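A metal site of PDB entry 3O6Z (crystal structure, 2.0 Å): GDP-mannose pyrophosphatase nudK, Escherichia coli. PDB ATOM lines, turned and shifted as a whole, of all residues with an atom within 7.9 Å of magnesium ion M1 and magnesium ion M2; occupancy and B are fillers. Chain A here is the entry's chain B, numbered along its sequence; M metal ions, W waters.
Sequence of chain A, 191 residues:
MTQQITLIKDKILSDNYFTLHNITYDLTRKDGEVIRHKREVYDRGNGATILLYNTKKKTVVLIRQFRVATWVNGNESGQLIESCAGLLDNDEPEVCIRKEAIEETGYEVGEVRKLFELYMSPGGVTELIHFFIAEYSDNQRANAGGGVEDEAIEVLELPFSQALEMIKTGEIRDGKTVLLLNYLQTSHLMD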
ATOM      1  N   ALA A  48     -10.126   5.587  -9.560  1.00  0.00           N
ATOM      2  CA  ALA A  48     -10.468   7.015  -9.593  1.00  0.00           C
ATOM      3  C   ALA A  48      -9.923   7.683  -8.356  1.00  0.00           C
ATOM      4  O   ALA A  48      -9.725   7.033  -7.329  1.00  0.00           O
ATOM      5  CB  ALA A  48     -12.011   7.201  -9.668  1.00  0.00           C
ATOM      6  N   ILE A  63      -5.953  12.341   2.415  1.00  0.00           N
ATOM      7  CA  ILE A  63      -5.967  11.229   3.383  1.00  0.00           C
ATOM      8  C   ILE A  63      -4.550  10.743   3.594  1.00  0.00           C
ATOM      9  O   ILE A  63      -3.650  11.132   2.864  1.00  0.00           O
ATOM     10  CB  ILE A  63      -6.882  10.027   2.959  1.00  0.00           C
ATOM     11  CG1 ILE A  63      -6.440   9.449   1.602  1.00  0.00           C
ATOM     12  CG2 ILE A  63      -8.387  10.442   2.961  1.00  0.00           C
ATOM     13  CD1 ILE A  63      -7.146   8.258   1.237  1.00  0.00           C
ATOM     14  N   GLN A  65      -2.660   6.990   4.854  1.00  0.00           N
ATOM     15  CA  GLN A  65      -2.747   5.588   5.264  1.00  0.00           C
ATOM     16  C   GLN A  65      -1.416   4.909   4.971  1.00  0.00           C
ATOM     17  O   GLN A  65      -0.604   5.431   4.208  1.00  0.00           O
ATOM     18  CB  GLN A  65      -3.882   4.873   4.503  1.00  0.00           C
ATOM     19  CG  GLN A  65      -3.571   4.554   3.054  1.00  0.00           C
ATOM     20  CD  GLN A  65      -4.805   4.354   2.233  1.00  0.00           C
ATOM     21  OE1 GLN A  65      -5.525   3.382   2.396  1.00  0.00           O
ATOM     22  NE2 GLN A  65      -5.064   5.300   1.334  1.00  0.00           N
ATOM     23  N   ARG A  67       0.952   2.471   3.278  1.00  0.00           N
ATOM     24  CA  ARG A  67       1.167   1.858   1.952  1.00  0.00           C
ATOM     25  C   ARG A  67       2.433   1.026   2.002  1.00  0.00           C
ATOM     26  O   ARG A  67       3.546   1.547   1.947  1.00  0.00           O
ATOM     27  CB  ARG A  67       1.329   2.927   0.870  1.00  0.00           C
ATOM     28  CG  ARG A  67       0.098   3.751   0.532  1.00  0.00           C
ATOM     29  CD  ARG A  67      -1.130   2.891   0.067  1.00  0.00           C
ATOM     30  NE  ARG A  67      -2.098   3.733  -0.655  1.00  0.00           N
ATOM     31  CZ  ARG A  67      -3.199   3.307  -1.248  1.00  0.00           C
ATOM     32  NH1 ARG A  67      -3.528   2.025  -1.191  1.00  0.00           N
ATOM     33  NH2 ARG A  67      -3.973   4.170  -1.887  1.00  0.00           N
ATOM     34  N   GLU A  82      -2.233  11.118   0.398  1.00  0.00           N
ATOM     35  CA  GLU A  82      -2.732  11.027  -0.980  1.00  0.00           C
ATOM     36  C   GLU A  82      -4.080  11.680  -1.064  1.00  0.00           C
ATOM     37  O   GLU A  82      -4.745  11.933  -0.041  1.00  0.00           O
ATOM     38  CB  GLU A  82      -2.910   9.570  -1.400  1.00  0.00           C
ATOM     39  CG  GLU A  82      -1.683   8.660  -1.326  1.00  0.00           C
ATOM     40  CD  GLU A  82      -2.100   7.202  -1.395  1.00  0.00           C
ATOM     41  OE1 GLU A  82      -2.805   6.844  -2.358  1.00  0.00           O
ATOM     42  OE2 GLU A  82      -1.778   6.427  -0.469  1.00  0.00           O
ATOM     43  N   SER A  83      -4.505  11.932  -2.282  1.00  0.00           N
ATOM     44  CA  SER A  83      -5.885  12.249  -2.520  1.00  0.00           C
ATOM     45  C   SER A  83      -6.692  10.953  -2.350  1.00  0.00           C
ATOM     46  O   SER A  83      -6.189   9.850  -2.616  1.00  0.00           O
ATOM     47  CB  SER A  83      -6.065  12.824  -3.935  1.00  0.00           C
ATOM     48  OG  SER A  83      -5.371  12.041  -4.880  1.00  0.00           O
ATOM     49  N   CYS A  84      -7.925  11.110  -1.844  1.00  0.00           N
ATOM     50  CA  CYS A  84      -8.899  10.024  -1.840  1.00  0.00           C
ATOM     51  C   CYS A  84      -8.955   9.322  -3.208  1.00  0.00           C
ATOM     52  O   CYS A  84      -9.036   9.983  -4.227  1.00  0.00           O
ATOM     53  CB  CYS A  84     -10.292  10.626  -1.531  1.00  0.00           C
ATOM     54  SG  CYS A  84     -11.656   9.436  -1.669  1.00  0.00           S
ATOM     55  N   ALA A  85      -8.957   7.981  -3.196  1.00  0.00           N
ATOM     56  CA  ALA A  85      -8.902   7.157  -4.410  1.00  0.00           C
ATOM     57  C   ALA A  85      -9.350   5.752  -4.122  1.00  0.00           C
ATOM     58  O   ALA A  85      -9.186   5.227  -3.013  1.00  0.00           O
ATOM     59  CB  ALA A  85      -7.439   7.055  -4.924  1.00  0.00           C
ATOM     60  N   GLY A  86      -9.852   5.085  -5.140  1.00  0.00           N
ATOM     61  CA  GLY A  86     -10.085   3.661  -4.981  1.00  0.00           C
ATOM     62  C   GLY A  86     -10.166   3.035  -6.336  1.00  0.00           C
ATOM     63  O   GLY A  86     -10.216   3.745  -7.362  1.00  0.00           O
ATOM     64  N   LEU A  87     -10.206   1.700  -6.339  1.00  0.00           N
ATOM     65  CA  LEU A  87     -10.355   0.928  -7.574  1.00  0.00           C
ATOM     66  C   LEU A  87     -11.809   0.964  -8.054  1.00  0.00           C
ATOM     67  O   LEU A  87     -12.740   0.940  -7.252  1.00  0.00           O
ATOM     68  CB  LEU A  87      -9.936  -0.524  -7.340  1.00  0.00           C
ATOM     69  CG  LEU A  87      -8.464  -0.796  -7.045  1.00  0.00           C
ATOM     70  CD1 LEU A  87      -8.310  -2.173  -6.456  1.00  0.00           C
ATOM     71  CD2 LEU A  87      -7.650  -0.694  -8.321  1.00  0.00           C
ATOM     72  N   CYS A  96     -17.919   5.159  -8.484  1.00  0.00           N
ATOM     73  CA  CYS A  96     -16.809   4.768  -7.647  1.00  0.00           C
ATOM     74  C   CYS A  96     -16.359   5.917  -6.751  1.00  0.00           C
ATOM     75  O   CYS A  96     -16.244   5.754  -5.537  1.00  0.00           O
ATOM     76  CB  CYS A  96     -15.637   4.222  -8.513  1.00  0.00           C
ATOM     77  SG  CYS A  96     -14.055   4.208  -7.698  1.00  0.00           S
ATOM     78  N   LYS A  99     -18.742   7.324  -3.753  1.00  0.00           N
ATOM     79  CA  LYS A  99     -18.631   6.207  -2.799  1.00  0.00           C
ATOM     80  C   LYS A  99     -17.322   6.226  -2.021  1.00  0.00           C
ATOM     81  O   LYS A  99     -17.332   6.272  -0.805  1.00  0.00           O
ATOM     82  CB  LYS A  99     -18.770   4.890  -3.561  1.00  0.00           C
ATOM     83  CG  LYS A  99     -18.904   3.647  -2.738  1.00  0.00           C
ATOM     84  CD  LYS A  99     -19.336   2.502  -3.667  1.00  0.00           C
ATOM     85  CE  LYS A  99     -19.076   1.139  -3.057  1.00  0.00           C
ATOM     86  NZ  LYS A  99     -19.590   0.050  -3.959  1.00  0.00           N
ATOM     87  N   GLU A 100     -16.174   6.178  -2.725  1.00  0.00           N
ATOM     88  CA  GLU A 100     -14.868   6.328  -2.051  1.00  0.00           C
ATOM     89  C   GLU A 100     -14.742   7.612  -1.211  1.00  0.00           C
ATOM     90  O   GLU A 100     -14.179   7.593  -0.100  1.00  0.00           O
ATOM     91  CB  GLU A 100     -13.675   6.253  -3.038  1.00  0.00           C
ATOM     92  CG  GLU A 100     -13.458   4.917  -3.751  1.00  0.00           C
ATOM     93  CD  GLU A 100     -13.022   3.771  -2.828  1.00  0.00           C
ATOM     94  OE1 GLU A 100     -12.437   4.020  -1.773  1.00  0.00           O
ATOM     95  OE2 GLU A 100     -13.259   2.605  -3.151  1.00  0.00           O
ATOM     96  N   ALA A 101     -15.245   8.730  -1.735  1.00  0.00           N
ATOM     97  CA  ALA A 101     -15.116   9.976  -0.972  1.00  0.00           C
ATOM     98  C   ALA A 101     -15.846   9.958   0.367  1.00  0.00           C
ATOM     99  O   ALA A 101     -15.267  10.396   1.356  1.00  0.00           O
ATOM    100  CB  ALA A 101     -15.550  11.196  -1.804  1.00  0.00           C
ATOM    101  N   GLU A 103     -16.755   7.244   2.124  1.00  0.00           N
ATOM    102  CA  GLU A 103     -16.150   6.197   2.950  1.00  0.00           C
ATOM    103  C   GLU A 103     -14.859   6.672   3.589  1.00  0.00           C
ATOM    104  O   GLU A 103     -14.682   6.562   4.793  1.00  0.00           O
ATOM    105  CB  GLU A 103     -15.881   4.950   2.132  1.00  0.00           C
ATOM    106  CG  GLU A 103     -17.154   4.251   1.654  1.00  0.00           C
ATOM    107  CD  GLU A 103     -16.835   2.993   0.849  1.00  0.00           C
ATOM    108  OE1 GLU A 103     -15.691   2.819   0.381  1.00  0.00           O
ATOM    109  OE2 GLU A 103     -17.764   2.187   0.672  1.00  0.00           O
ATOM    110  N   GLU A 104     -13.983   7.216   2.752  1.00  0.00           N
ATOM    111  CA  GLU A 104     -12.659   7.646   3.178  1.00  0.00           C
ATOM    112  C   GLU A 104     -12.613   9.011   3.865  1.00  0.00           C
ATOM    113  O   GLU A 104     -11.879   9.177   4.850  1.00  0.00           O
ATOM    114  CB  GLU A 104     -11.675   7.549   2.018  1.00  0.00           C
ATOM    115  CG  GLU A 104     -11.717   6.176   1.320  1.00  0.00           C
ATOM    116  CD  GLU A 104     -10.514   5.907   0.437  1.00  0.00           C
ATOM    117  OE1 GLU A 104      -9.754   6.833   0.141  1.00  0.00           O
ATOM    118  OE2 GLU A 104     -10.331   4.738   0.005  1.00  0.00           O
ATOM    119  N   GLY A 146     -12.471   7.676   7.243  1.00  0.00           N
ATOM    120  CA  GLY A 146     -11.579   6.634   7.814  1.00  0.00           C
ATOM    121  C   GLY A 146     -11.541   5.279   7.109  1.00  0.00           C
ATOM    122  O   GLY A 146     -10.794   4.357   7.509  1.00  0.00           O
ATOM    123  N   GLY A 147     -12.326   5.162   6.034  1.00  0.00           N
ATOM    124  CA  GLY A 147     -12.462   3.910   5.292  1.00  0.00           C
ATOM    125  C   GLY A 147     -13.404   2.888   5.930  1.00  0.00           C
ATOM    126  O   GLY A 147     -13.993   3.148   6.986  1.00  0.00           O
ATOM    127  N   VAL A 148     -13.536   1.747   5.263  1.00  0.00           N
ATOM    128  CA  VAL A 148     -14.397   0.653   5.659  1.00  0.00           C
ATOM    129  C   VAL A 148     -13.606  -0.640   5.518  1.00  0.00           C
ATOM    130  O   VAL A 148     -12.470  -0.620   5.016  1.00  0.00           O
ATOM    131  CB  VAL A 148     -15.637   0.548   4.739  1.00  0.00           C
ATOM    132  CG1 VAL A 148     -16.543   1.740   4.942  1.00  0.00           C
ATOM    133  CG2 VAL A 148     -15.217   0.415   3.293  1.00  0.00           C
ATOM    134  N   GLU A 151      -9.668  -1.014   5.814  1.00  0.00           N
ATOM    135  CA  GLU A 151      -8.983   0.255   5.594  1.00  0.00           C
ATOM    136  C   GLU A 151      -8.702   0.948   6.924  1.00  0.00           C
ATOM    137  O   GLU A 151      -9.464   0.821   7.867  1.00  0.00           O
ATOM    138  CB  GLU A 151      -9.800   1.181   4.694  1.00  0.00           C
ATOM    139  CG  GLU A 151      -9.754   0.830   3.220  1.00  0.00           C
ATOM    140  CD  GLU A 151     -10.686   1.681   2.424  1.00  0.00           C
ATOM    141  OE1 GLU A 151     -11.845   1.931   2.863  1.00  0.00           O
ATOM    142  OE2 GLU A 151     -10.255   2.084   1.323  1.00  0.00           O
ATOM    143  N   ILE A 153      -7.624   4.741   7.619  1.00  0.00           N
ATOM    144  CA  ILE A 153      -7.370   6.004   6.938  1.00  0.00           C
ATOM    145  C   ILE A 153      -7.508   7.199   7.887  1.00  0.00           C
ATOM    146  O   ILE A 153      -8.494   7.329   8.625  1.00  0.00           O
ATOM    147  CB  ILE A 153      -8.322   6.149   5.725  1.00  0.00           C
ATOM    148  CG1 ILE A 153      -7.923   5.177   4.615  1.00  0.00           C
ATOM    149  CG2 ILE A 153      -8.365   7.604   5.236  1.00  0.00           C
ATOM    150  CD1 ILE A 153      -8.887   5.080   3.462  1.00  0.00           C
ATOM    151  N   LYS A 176      -0.468  11.017  -8.334  1.00  0.00           N
ATOM    152  CA  LYS A 176      -1.817  11.570  -8.554  1.00  0.00           C
ATOM    153  C   LYS A 176      -2.147  12.810  -7.679  1.00  0.00           C
ATOM    154  O   LYS A 176      -2.874  13.688  -8.098  1.00  0.00           O
ATOM    155  CB  LYS A 176      -2.912  10.501  -8.351  1.00  0.00           C
ATOM    156  CG  LYS A 176      -3.152  10.107  -6.874  1.00  0.00           C
ATOM    157  CD  LYS A 176      -3.980   8.828  -6.730  1.00  0.00           C
ATOM    158  CE  LYS A 176      -3.974   8.360  -5.311  1.00  0.00           C
ATOM    159  NZ  LYS A 176      -2.661   7.786  -4.898  1.00  0.00           N
HETATM  160 MG    MG M   1     -11.349   3.133  -0.392  1.00  0.00          MG
HETATM  161 MG    MG M   2      -8.444   4.066  -1.182  1.00  0.00          MG
HETATM  162  O   HOH W   1      -9.838   2.579  -1.490  1.00  0.00           O
HETATM  163  O   HOH W   2     -12.184   1.234  -1.152  1.00  0.00           O
HETATM  164  O   HOH W   3      -7.785   2.841   0.842  1.00  0.00           O
HETATM  165  O   HOH W   4     -13.064   3.373   1.134  1.00  0.00           O
HETATM  166  O   HOH W   5      -6.664   3.446  -2.675  1.00  0.00           O
HETATM  167  O   HOH W   6      -7.201   5.760  -0.505  1.00  0.00           O
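Magnesium ion M1 is bound by the side-chain carboxylate (OE2) of Glu 104 (1.9 Å), water W1 (1.9 Å), the side-chain carboxylate (OE1) of Glu 100 (2.0 Å), water W2 (2.2 Å), the side-chain carboxylate (OE2) of Glu 151 (2.3 Å) and water W4 (2.3 Å).
Magnesium ion M2 is bound by water W1 (2.1 Å), water W6 (2.2 Å), O of Ala 85 (2.3 Å), OE2 of Glu 104 (2.3 Å), water W5 (2.4 Å) and water W3 (2.5 Å).
Magnesium ion M2 has six donor atoms within binding distance.
The side-chain sulfur (SG) of Cys 84 lies within hydrogen-bond range of the side-chain carboxylate (OE1) of Glu 104 (3.7 Å).
The backbone carbonyl oxygen (O) of Glu 104 lies within hydrogen-bond range of the backbone NH (N) of Gly 146 (2.9 Å).
O of Glu 100 is in hydrogen-bond range of SG of Cys 84 (3.5 Å).
The backbone NH (N) of Val 148 sits at hydrogen-bond distance from the side-chain carboxylate (OE1) of Glu 151 (2.9 Å).
Within 4 Å of magnesium ion M2: Ala 85, Glu 104 and Glu 151.
Water W4 lies within hydrogen-bond range of the side-chain carboxylate (OE1) of Glu 151 (2.6 Å) and the side-chain carboxylate (OE1) of Glu 103 (2.8 Å).
Water W6 bridges OE1 of Glu 104 and NE2 of Gln 65.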
